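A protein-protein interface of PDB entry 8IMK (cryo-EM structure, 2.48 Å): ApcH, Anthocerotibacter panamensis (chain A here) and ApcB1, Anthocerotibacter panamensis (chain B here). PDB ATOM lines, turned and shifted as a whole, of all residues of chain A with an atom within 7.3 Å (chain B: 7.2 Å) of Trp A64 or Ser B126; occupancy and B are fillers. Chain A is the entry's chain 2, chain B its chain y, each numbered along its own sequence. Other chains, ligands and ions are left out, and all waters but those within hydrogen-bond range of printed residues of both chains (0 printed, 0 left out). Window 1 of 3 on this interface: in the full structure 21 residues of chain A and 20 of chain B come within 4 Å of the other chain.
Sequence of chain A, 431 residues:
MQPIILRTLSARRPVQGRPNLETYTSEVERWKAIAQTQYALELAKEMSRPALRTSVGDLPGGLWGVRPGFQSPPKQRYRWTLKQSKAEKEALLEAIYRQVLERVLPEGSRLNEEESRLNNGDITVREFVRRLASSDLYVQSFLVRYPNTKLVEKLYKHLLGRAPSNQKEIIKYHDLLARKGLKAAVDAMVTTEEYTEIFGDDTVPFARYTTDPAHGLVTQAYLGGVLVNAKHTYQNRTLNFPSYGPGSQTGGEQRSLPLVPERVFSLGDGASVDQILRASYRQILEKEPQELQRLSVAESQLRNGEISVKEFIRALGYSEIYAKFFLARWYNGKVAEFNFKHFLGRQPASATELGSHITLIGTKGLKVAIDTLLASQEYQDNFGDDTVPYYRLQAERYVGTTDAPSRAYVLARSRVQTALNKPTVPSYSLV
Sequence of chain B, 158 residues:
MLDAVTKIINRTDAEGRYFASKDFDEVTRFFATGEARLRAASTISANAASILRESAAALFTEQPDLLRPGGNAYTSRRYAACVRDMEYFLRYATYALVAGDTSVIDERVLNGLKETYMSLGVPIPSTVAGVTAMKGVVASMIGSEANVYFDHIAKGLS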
ATOM      1  N   LEU A  52     -15.853  26.807   5.998  1.00  0.00           N
ATOM      2  CA  LEU A  52     -16.787  26.413   4.937  1.00  0.00           C
ATOM      3  C   LEU A  52     -18.131  27.111   5.134  1.00  0.00           C
ATOM      4  O   LEU A  52     -19.184  26.478   5.093  1.00  0.00           O
ATOM      5  CB  LEU A  52     -16.954  24.898   4.903  1.00  0.00           C
ATOM      6  CG  LEU A  52     -15.786  24.119   4.309  1.00  0.00           C
ATOM      7  CD1 LEU A  52     -15.816  22.678   4.754  1.00  0.00           C
ATOM      8  CD2 LEU A  52     -15.821  24.215   2.800  1.00  0.00           C
ATOM      9  N   LEU A  59     -19.310  27.209  -4.902  1.00  0.00           N
ATOM     10  CA  LEU A  59     -19.609  26.085  -5.768  1.00  0.00           C
ATOM     11  C   LEU A  59     -20.032  24.882  -4.927  1.00  0.00           C
ATOM     12  O   LEU A  59     -19.562  24.709  -3.801  1.00  0.00           O
ATOM     13  CB  LEU A  59     -18.399  25.715  -6.614  1.00  0.00           C
ATOM     14  CG  LEU A  59     -18.107  26.641  -7.792  1.00  0.00           C
ATOM     15  CD1 LEU A  59     -16.915  26.130  -8.601  1.00  0.00           C
ATOM     16  CD2 LEU A  59     -19.331  26.899  -8.645  1.00  0.00           C
ATOM     17  N   PRO A  60     -20.925  24.045  -5.443  1.00  0.00           N
ATOM     18  CA  PRO A  60     -21.296  22.834  -4.704  1.00  0.00           C
ATOM     19  C   PRO A  60     -20.105  21.903  -4.542  1.00  0.00           C
ATOM     20  O   PRO A  60     -19.268  21.768  -5.435  1.00  0.00           O
ATOM     21  CB  PRO A  60     -22.385  22.203  -5.577  1.00  0.00           C
ATOM     22  CG  PRO A  60     -22.221  22.815  -6.911  1.00  0.00           C
ATOM     23  CD  PRO A  60     -21.664  24.175  -6.707  1.00  0.00           C
ATOM     24  N   GLY A  61     -20.038  21.252  -3.384  1.00  0.00           N
ATOM     25  CA  GLY A  61     -18.963  20.331  -3.077  1.00  0.00           C
ATOM     26  C   GLY A  61     -18.121  20.696  -1.877  1.00  0.00           C
ATOM     27  O   GLY A  61     -17.274  19.890  -1.479  1.00  0.00           O
ATOM     28  N   GLY A  62     -18.305  21.874  -1.298  1.00  0.00           N
ATOM     29  CA  GLY A  62     -17.599  22.220  -0.073  1.00  0.00           C
ATOM     30  C   GLY A  62     -16.103  22.330  -0.277  1.00  0.00           C
ATOM     31  O   GLY A  62     -15.621  23.172  -1.038  1.00  0.00           O
ATOM     32  N   LEU A  63     -15.348  21.467   0.409  1.00  0.00           N
ATOM     33  CA  LEU A  63     -13.903  21.406   0.204  1.00  0.00           C
ATOM     34  C   LEU A  63     -13.562  21.058  -1.236  1.00  0.00           C
ATOM     35  O   LEU A  63     -12.446  21.309  -1.696  1.00  0.00           O
ATOM     36  CB  LEU A  63     -13.272  20.374   1.137  1.00  0.00           C
ATOM     37  CG  LEU A  63     -13.183  20.609   2.638  1.00  0.00           C
ATOM     38  CD1 LEU A  63     -12.744  19.330   3.318  1.00  0.00           C
ATOM     39  CD2 LEU A  63     -12.206  21.722   2.934  1.00  0.00           C
ATOM     40  N   TRP A  64     -14.504  20.458  -1.955  1.00  0.00           N
ATOM     41  CA  TRP A  64     -14.294  20.025  -3.326  1.00  0.00           C
ATOM     42  C   TRP A  64     -15.169  20.788  -4.308  1.00  0.00           C
ATOM     43  O   TRP A  64     -15.562  20.248  -5.344  1.00  0.00           O
ATOM     44  CB  TRP A  64     -14.525  18.521  -3.424  1.00  0.00           C
ATOM     45  CG  TRP A  64     -13.490  17.776  -2.658  1.00  0.00           C
ATOM     46  CD1 TRP A  64     -13.616  17.237  -1.415  1.00  0.00           C
ATOM     47  CD2 TRP A  64     -12.147  17.521  -3.071  1.00  0.00           C
ATOM     48  NE1 TRP A  64     -12.442  16.652  -1.034  1.00  0.00           N
ATOM     49  CE2 TRP A  64     -11.520  16.813  -2.033  1.00  0.00           C
ATOM     50  CE3 TRP A  64     -11.413  17.821  -4.221  1.00  0.00           C
ATOM     51  CZ2 TRP A  64     -10.195  16.389  -2.114  1.00  0.00           C
ATOM     52  CZ3 TRP A  64     -10.104  17.406  -4.296  1.00  0.00           C
ATOM     53  CH2 TRP A  64      -9.507  16.697  -3.251  1.00  0.00           C
ATOM     54  N   GLY A  65     -15.484  22.039  -3.998  1.00  0.00           N
ATOM     55  CA  GLY A  65     -16.288  22.866  -4.869  1.00  0.00           C
ATOM     56  C   GLY A  65     -15.467  23.480  -5.978  1.00  0.00           C
ATOM     57  O   GLY A  65     -15.367  24.702  -6.091  1.00  0.00           O
ATOM     58  N   VAL A  66     -14.859  22.633  -6.802  1.00  0.00           N
ATOM     59  CA  VAL A  66     -14.032  23.083  -7.909  1.00  0.00           C
ATOM     60  C   VAL A  66     -14.489  22.341  -9.153  1.00  0.00           C
ATOM     61  O   VAL A  66     -15.068  21.256  -9.072  1.00  0.00           O
ATOM     62  CB  VAL A  66     -12.524  22.857  -7.643  1.00  0.00           C
ATOM     63  CG1 VAL A  66     -12.113  23.468  -6.331  1.00  0.00           C
ATOM     64  CG2 VAL A  66     -12.181  21.389  -7.678  1.00  0.00           C
ATOM     65  N   ARG A  67     -14.241  22.940 -10.311  1.00  0.00           N
ATOM     66  CA  ARG A  67     -14.626  22.359 -11.576  1.00  0.00           C
ATOM     67  C   ARG A  67     -13.582  22.803 -12.592  1.00  0.00           C
ATOM     68  O   ARG A  67     -13.413  24.011 -12.806  1.00  0.00           O
ATOM     69  CB  ARG A  67     -16.027  22.793 -12.007  1.00  0.00           C
ATOM     70  CG  ARG A  67     -16.612  21.993 -13.147  1.00  0.00           C
ATOM     71  CD  ARG A  67     -17.048  20.621 -12.700  1.00  0.00           C
ATOM     72  NE  ARG A  67     -17.479  19.770 -13.808  1.00  0.00           N
ATOM     73  CZ  ARG A  67     -18.533  19.999 -14.588  1.00  0.00           C
ATOM     74  NH1 ARG A  67     -19.302  21.062 -14.398  1.00  0.00           N
ATOM     75  NH2 ARG A  67     -18.819  19.153 -15.565  1.00  0.00           N
ATOM     76  N   TYR A 209     -25.522  17.948  -8.407  1.00  0.00           N
ATOM     77  CA  TYR A 209     -24.961  18.179  -7.088  1.00  0.00           C
ATOM     78  C   TYR A 209     -25.988  18.239  -5.970  1.00  0.00           C
ATOM     79  O   TYR A 209     -25.600  18.401  -4.810  1.00  0.00           O
ATOM     80  CB  TYR A 209     -24.153  19.478  -7.076  1.00  0.00           C
ATOM     81  CG  TYR A 209     -22.943  19.473  -7.966  1.00  0.00           C
ATOM     82  CD1 TYR A 209     -21.725  18.995  -7.510  1.00  0.00           C
ATOM     83  CD2 TYR A 209     -23.006  19.978  -9.252  1.00  0.00           C
ATOM     84  CE1 TYR A 209     -20.609  19.001  -8.320  1.00  0.00           C
ATOM     85  CE2 TYR A 209     -21.899  19.988 -10.067  1.00  0.00           C
ATOM     86  CZ  TYR A 209     -20.702  19.501  -9.595  1.00  0.00           C
ATOM     87  OH  TYR A 209     -19.595  19.511 -10.405  1.00  0.00           O
ATOM     88  N   LEU A 223     -21.154  12.016  -3.271  1.00  0.00           N
ATOM     89  CA  LEU A 223     -19.745  12.091  -2.915  1.00  0.00           C
ATOM     90  C   LEU A 223     -18.856  11.693  -4.082  1.00  0.00           C
ATOM     91  O   LEU A 223     -17.879  12.386  -4.399  1.00  0.00           O
ATOM     92  CB  LEU A 223     -19.478  11.193  -1.712  1.00  0.00           C
ATOM     93  CG  LEU A 223     -18.103  11.309  -1.067  1.00  0.00           C
ATOM     94  CD1 LEU A 223     -18.003  12.607  -0.315  1.00  0.00           C
ATOM     95  CD2 LEU A 223     -17.870  10.138  -0.141  1.00  0.00           C
ATOM     96  N   VAL A 226     -18.964  14.483  -6.803  1.00  0.00           N
ATOM     97  CA  VAL A 226     -18.156  15.665  -6.522  1.00  0.00           C
ATOM     98  C   VAL A 226     -16.670  15.329  -6.582  1.00  0.00           C
ATOM     99  O   VAL A 226     -15.850  16.183  -6.928  1.00  0.00           O
ATOM    100  CB  VAL A 226     -18.539  16.323  -5.179  1.00  0.00           C
ATOM    101  CG1 VAL A 226     -20.000  16.700  -5.165  1.00  0.00           C
ATOM    102  CG2 VAL A 226     -18.193  15.450  -4.002  1.00  0.00           C
ATOM    103  N   LEU A 227     -16.289  14.096  -6.248  1.00  0.00           N
ATOM    104  CA  LEU A 227     -14.872  13.752  -6.300  1.00  0.00           C
ATOM    105  C   LEU A 227     -14.378  13.589  -7.735  1.00  0.00           C
ATOM    106  O   LEU A 227     -13.273  14.028  -8.067  1.00  0.00           O
ATOM    107  CB  LEU A 227     -14.594  12.497  -5.481  1.00  0.00           C
ATOM    108  CG  LEU A 227     -14.730  12.743  -3.979  1.00  0.00           C
ATOM    109  CD1 LEU A 227     -14.470  11.480  -3.181  1.00  0.00           C
ATOM    110  CD2 LEU A 227     -13.812  13.870  -3.546  1.00  0.00           C
ATOM    111  N   ASN A 229     -15.903  14.830 -10.434  1.00  0.00           N
ATOM    112  CA  ASN A 229     -16.170  16.057 -11.164  1.00  0.00           C
ATOM    113  C   ASN A 229     -15.194  17.163 -10.819  1.00  0.00           C
ATOM    114  O   ASN A 229     -15.151  18.169 -11.529  1.00  0.00           O
ATOM    115  CB  ASN A 229     -17.599  16.521 -10.904  1.00  0.00           C
ATOM    116  CG  ASN A 229     -18.608  15.785 -11.751  1.00  0.00           C
ATOM    117  OD1 ASN A 229     -18.410  15.605 -12.945  1.00  0.00           O
ATOM    118  ND2 ASN A 229     -19.693  15.347 -11.135  1.00  0.00           N
ATOM    119  N   ALA A 230     -14.420  17.006  -9.753  1.00  0.00           N
ATOM    120  CA  ALA A 230     -13.374  17.950  -9.407  1.00  0.00           C
ATOM    121  C   ALA A 230     -12.078  17.686 -10.156  1.00  0.00           C
ATOM    122  O   ALA A 230     -11.202  18.554 -10.178  1.00  0.00           O
ATOM    123  CB  ALA A 230     -13.120  17.905  -7.900  1.00  0.00           C
ATOM    124  N   LYS A 231     -11.949  16.529 -10.787  1.00  0.00           N
ATOM    125  CA  LYS A 231     -10.695  16.089 -11.369  1.00  0.00           C
ATOM    126  C   LYS A 231     -10.589  16.561 -12.808  1.00  0.00           C
ATOM    127  O   LYS A 231     -11.581  16.598 -13.539  1.00  0.00           O
ATOM    128  CB  LYS A 231     -10.577  14.568 -11.313  1.00  0.00           C
ATOM    129  CG  LYS A 231     -10.190  14.031  -9.964  1.00  0.00           C
ATOM    130  CD  LYS A 231     -10.402  12.537  -9.891  1.00  0.00           C
ATOM    131  CE  LYS A 231     -10.322  12.036  -8.464  1.00  0.00           C
ATOM    132  NZ  LYS A 231      -9.217  12.677  -7.706  1.00  0.00           N
ATOM    133  N   GLN A 235      -6.294  13.304 -15.044  1.00  0.00           N
ATOM    134  CA  GLN A 235      -5.607  13.734 -13.832  1.00  0.00           C
ATOM    135  C   GLN A 235      -4.766  12.604 -13.259  1.00  0.00           C
ATOM    136  O   GLN A 235      -3.670  12.834 -12.737  1.00  0.00           O
ATOM    137  CB  GLN A 235      -6.607  14.239 -12.793  1.00  0.00           C
ATOM    138  CG  GLN A 235      -5.940  14.648 -11.502  1.00  0.00           C
ATOM    139  CD  GLN A 235      -6.720  15.660 -10.709  1.00  0.00           C
ATOM    140  OE1 GLN A 235      -7.496  16.434 -11.256  1.00  0.00           O
ATOM    141  NE2 GLN A 235      -6.502  15.677  -9.408  1.00  0.00           N
ATOM    142  N   LEU B  59      -0.194  20.772  -0.224  1.00  0.00           N
ATOM    143  CA  LEU B  59      -1.494  20.321   0.262  1.00  0.00           C
ATOM    144  C   LEU B  59      -2.336  21.487   0.752  1.00  0.00           C
ATOM    145  O   LEU B  59      -3.527  21.582   0.438  1.00  0.00           O
ATOM    146  CB  LEU B  59      -1.316  19.301   1.383  1.00  0.00           C
ATOM    147  CG  LEU B  59      -2.576  18.948   2.176  1.00  0.00           C
ATOM    148  CD1 LEU B  59      -3.635  18.340   1.282  1.00  0.00           C
ATOM    149  CD2 LEU B  59      -2.236  18.003   3.308  1.00  0.00           C
ATOM    150  N   GLU B  62      -3.500  23.923  -1.968  1.00  0.00           N
ATOM    151  CA  GLU B  62      -4.645  23.417  -2.718  1.00  0.00           C
ATOM    152  C   GLU B  62      -5.936  23.542  -1.918  1.00  0.00           C
ATOM    153  O   GLU B  62      -6.987  23.873  -2.478  1.00  0.00           O
ATOM    154  CB  GLU B  62      -4.407  21.965  -3.127  1.00  0.00           C
ATOM    155  CG  GLU B  62      -5.575  21.317  -3.851  1.00  0.00           C
ATOM    156  CD  GLU B  62      -5.138  20.242  -4.829  1.00  0.00           C
ATOM    157  OE1 GLU B  62      -5.802  19.184  -4.881  1.00  0.00           O
ATOM    158  OE2 GLU B  62      -4.139  20.457  -5.548  1.00  0.00           O
ATOM    159  N   GLN B  63      -5.887  23.271  -0.616  1.00  0.00           N
ATOM    160  CA  GLN B  63      -7.070  23.269   0.242  1.00  0.00           C
ATOM    161  C   GLN B  63      -6.799  24.132   1.464  1.00  0.00           C
ATOM    162  O   GLN B  63      -6.427  23.625   2.529  1.00  0.00           O
ATOM    163  CB  GLN B  63      -7.459  21.848   0.644  1.00  0.00           C
ATOM    164  CG  GLN B  63      -7.687  20.935  -0.535  1.00  0.00           C
ATOM    165  CD  GLN B  63      -8.569  19.766  -0.195  1.00  0.00           C
ATOM    166  OE1 GLN B  63      -8.530  19.254   0.916  1.00  0.00           O
ATOM    167  NE2 GLN B  63      -9.380  19.339  -1.149  1.00  0.00           N
ATOM    168  N   ASP B  65      -8.883  25.582   3.356  1.00  0.00           N
ATOM    169  CA  ASP B  65      -9.926  25.514   4.373  1.00  0.00           C
ATOM    170  C   ASP B  65      -9.555  24.556   5.493  1.00  0.00           C
ATOM    171  O   ASP B  65     -10.143  24.604   6.578  1.00  0.00           O
ATOM    172  CB  ASP B  65     -11.250  25.106   3.736  1.00  0.00           C
ATOM    173  CG  ASP B  65     -11.817  26.178   2.836  1.00  0.00           C
ATOM    174  OD1 ASP B  65     -11.556  27.370   3.093  1.00  0.00           O
ATOM    175  OD2 ASP B  65     -12.530  25.834   1.871  1.00  0.00           O
ATOM    176  N   LEU B  66      -8.586  23.673   5.253  1.00  0.00           N
ATOM    177  CA  LEU B  66      -8.143  22.765   6.303  1.00  0.00           C
ATOM    178  C   LEU B  66      -7.440  23.519   7.425  1.00  0.00           C
ATOM    179  O   LEU B  66      -7.495  23.107   8.586  1.00  0.00           O
ATOM    180  CB  LEU B  66      -7.226  21.692   5.716  1.00  0.00           C
ATOM    181  CG  LEU B  66      -7.785  20.789   4.615  1.00  0.00           C
ATOM    182  CD1 LEU B  66      -6.652  20.088   3.903  1.00  0.00           C
ATOM    183  CD2 LEU B  66      -8.762  19.779   5.171  1.00  0.00           C
ATOM    184  N   VAL B 122     -10.919  12.786   9.988  1.00  0.00           N
ATOM    185  CA  VAL B 122      -9.900  13.214   9.026  1.00  0.00           C
ATOM    186  C   VAL B 122     -10.442  13.039   7.617  1.00  0.00           C
ATOM    187  O   VAL B 122     -10.928  11.946   7.274  1.00  0.00           O
ATOM    188  CB  VAL B 122      -8.609  12.399   9.207  1.00  0.00           C
ATOM    189  CG1 VAL B 122      -7.672  12.672   8.067  1.00  0.00           C
ATOM    190  CG2 VAL B 122      -7.948  12.713  10.524  1.00  0.00           C
ATOM    191  N   PRO B 123     -10.382  14.056   6.755  1.00  0.00           N
ATOM    192  CA  PRO B 123     -10.886  13.892   5.384  1.00  0.00           C
ATOM    193  C   PRO B 123      -9.937  13.028   4.568  1.00  0.00           C
ATOM    194  O   PRO B 123      -8.778  13.385   4.357  1.00  0.00           O
ATOM    195  CB  PRO B 123     -10.948  15.327   4.852  1.00  0.00           C
ATOM    196  CG  PRO B 123     -10.053  16.112   5.711  1.00  0.00           C
ATOM    197  CD  PRO B 123      -9.776  15.377   6.977  1.00  0.00           C
ATOM    198  N   ILE B 124     -10.432  11.872   4.127  1.00  0.00           N
ATOM    199  CA  ILE B 124      -9.595  10.958   3.346  1.00  0.00           C
ATOM    200  C   ILE B 124      -9.229  11.517   1.979  1.00  0.00           C
ATOM    201  O   ILE B 124      -8.061  11.405   1.590  1.00  0.00           O
ATOM    202  CB  ILE B 124     -10.244   9.569   3.291  1.00  0.00           C
ATOM    203  CG1 ILE B 124     -10.058   8.864   4.636  1.00  0.00           C
ATOM    204  CG2 ILE B 124      -9.693   8.750   2.145  1.00  0.00           C
ATOM    205  CD1 ILE B 124     -10.885   7.625   4.816  1.00  0.00           C
ATOM    206  N   PRO B 125     -10.140  12.103   1.193  1.00  0.00           N
ATOM    207  CA  PRO B 125      -9.707  12.661  -0.100  1.00  0.00           C
ATOM    208  C   PRO B 125      -8.658  13.753   0.020  1.00  0.00           C
ATOM    209  O   PRO B 125      -7.756  13.828  -0.820  1.00  0.00           O
ATOM    210  CB  PRO B 125     -11.018  13.176  -0.703  1.00  0.00           C
ATOM    211  CG  PRO B 125     -12.050  12.336  -0.082  1.00  0.00           C
ATOM    212  CD  PRO B 125     -11.605  12.148   1.319  1.00  0.00           C
ATOM    213  N   SER B 126      -8.737  14.596   1.049  1.00  0.00           N
ATOM    214  CA  SER B 126      -7.688  15.586   1.270  1.00  0.00           C
ATOM    215  C   SER B 126      -6.362  14.921   1.615  1.00  0.00           C
ATOM    216  O   SER B 126      -5.299  15.368   1.173  1.00  0.00           O
ATOM    217  CB  SER B 126      -8.100  16.553   2.373  1.00  0.00           C
ATOM    218  OG  SER B 126      -9.184  17.362   1.965  1.00  0.00           O
ATOM    219  N   THR B 127      -6.407  13.848   2.406  1.00  0.00           N
ATOM    220  CA  THR B 127      -5.186  13.123   2.735  1.00  0.00           C
ATOM    221  C   THR B 127      -4.576  12.489   1.493  1.00  0.00           C
ATOM    222  O   THR B 127      -3.351  12.465   1.338  1.00  0.00           O
ATOM    223  CB  THR B 127      -5.473  12.055   3.788  1.00  0.00           C
ATOM    224  OG1 THR B 127      -6.301  12.608   4.812  1.00  0.00           O
ATOM    225  CG2 THR B 127      -4.184  11.568   4.416  1.00  0.00           C
ATOM    226  N   VAL B 128      -5.415  11.964   0.601  1.00  0.00           N
ATOM    227  CA  VAL B 128      -4.921  11.380  -0.639  1.00  0.00           C
ATOM    228  C   VAL B 128      -4.334  12.459  -1.536  1.00  0.00           C
ATOM    229  O   VAL B 128      -3.336  12.236  -2.224  1.00  0.00           O
ATOM    230  CB  VAL B 128      -6.041  10.592  -1.344  1.00  0.00           C
ATOM    231  CG1 VAL B 128      -5.620  10.196  -2.745  1.00  0.00           C
ATOM    232  CG2 VAL B 128      -6.410   9.361  -0.539  1.00  0.00           C
ATOM    233  N   ALA B 129      -4.936  13.650  -1.535  1.00  0.00           N
ATOM    234  CA  ALA B 129      -4.364  14.770  -2.275  1.00  0.00           C
ATOM    235  C   ALA B 129      -2.992  15.154  -1.733  1.00  0.00           C
ATOM    236  O   ALA B 129      -2.076  15.457  -2.502  1.00  0.00           O
ATOM    237  CB  ALA B 129      -5.314  15.963  -2.228  1.00  0.00           C
ATOM    238  N   GLY B 130      -2.832  15.150  -0.411  1.00  0.00           N
ATOM    239  CA  GLY B 130      -1.522  15.410   0.165  1.00  0.00           C
ATOM    240  C   GLY B 130      -0.501  14.336  -0.167  1.00  0.00           C
ATOM    241  O   GLY B 130       0.658  14.635  -0.467  1.00  0.00           O
ATOM    242  N   VAL B 131      -0.915  13.070  -0.095  1.00  0.00           N
ATOM    243  CA  VAL B 131      -0.043  11.962  -0.479  1.00  0.00           C
ATOM    244  C   VAL B 131       0.369  12.098  -1.934  1.00  0.00           C
ATOM    245  O   VAL B 131       1.520  11.845  -2.297  1.00  0.00           O
ATOM    246  CB  VAL B 131      -0.747  10.618  -0.211  1.00  0.00           C
ATOM    247  CG1 VAL B 131      -0.028   9.475  -0.908  1.00  0.00           C
ATOM    248  CG2 VAL B 131      -0.827  10.356   1.266  1.00  0.00           C
ATOM    249  N   THR B 132      -0.564  12.516  -2.784  1.00  0.00           N
ATOM    250  CA  THR B 132      -0.268  12.689  -4.197  1.00  0.00           C
ATOM    251  C   THR B 132       0.689  13.851  -4.423  1.00  0.00           C
ATOM    252  O   THR B 132       1.568  13.785  -5.290  1.00  0.00           O
ATOM    253  CB  THR B 132      -1.571  12.898  -4.959  1.00  0.00           C
ATOM    254  OG1 THR B 132      -2.385  11.729  -4.827  1.00  0.00           O
ATOM    255  CG2 THR B 132      -1.282  13.094  -6.392  1.00  0.00           C
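Of chain B, only Gln B63 (3.2 Å), Pro B125 (3.6 Å) and Ser B126 (3.9 Å) come within 4 Å of Trp A64.
Ser B126 touches just one residue of chain A: Trp A64 (3.9 Å).
Of the printed residues of chain A, Gln B63 touches Leu A63 and Trp A64.
Of the printed residues of chain B, Leu A52 touches Asp B65 (3.8 Å).
Ile B124 touches none of the printed residues of chain A.
Val A66 touches none of the printed residues of chain B.
The nearest residue of chain B that does not touch Trp A64 is Ala B129 (4.4 Å).
The nearest printed residue of chain A that does not touch Gln B63 is Val A66 (7.2 Å).
Of the 18 printed residues of chain A, 3 touch a printed residue of chain B.
Printed residues of chain A that touch a printed residue of chain B: Leu A52, Leu A63 and Trp A64.
Hydrophobic or aromatic side chains of chain A within 4 Å of the printed part of chain B: Leu A52, Leu A63 and Trp A64.
Printed residues of chain B that touch a printed residue of chain A: Gln B63, Asp B65, Pro B125 and Ser B126.
Along chain B the printed residues that touch a printed residue of chain A span positions 63 to 126.
Among the printed residues, no Asp or Glu carboxylate lies within 4 Å of a Lys or Arg side-chain nitrogen of the other chain.
Among the printed residues, pairs that only touch across the chains: Leu A52 with Asp B65, Leu A63 with Gln B63, Leu A63 with Asp B65, Trp A64 with Gln B63, Trp A64 with Pro B125 and Trp A64 with Ser B126.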
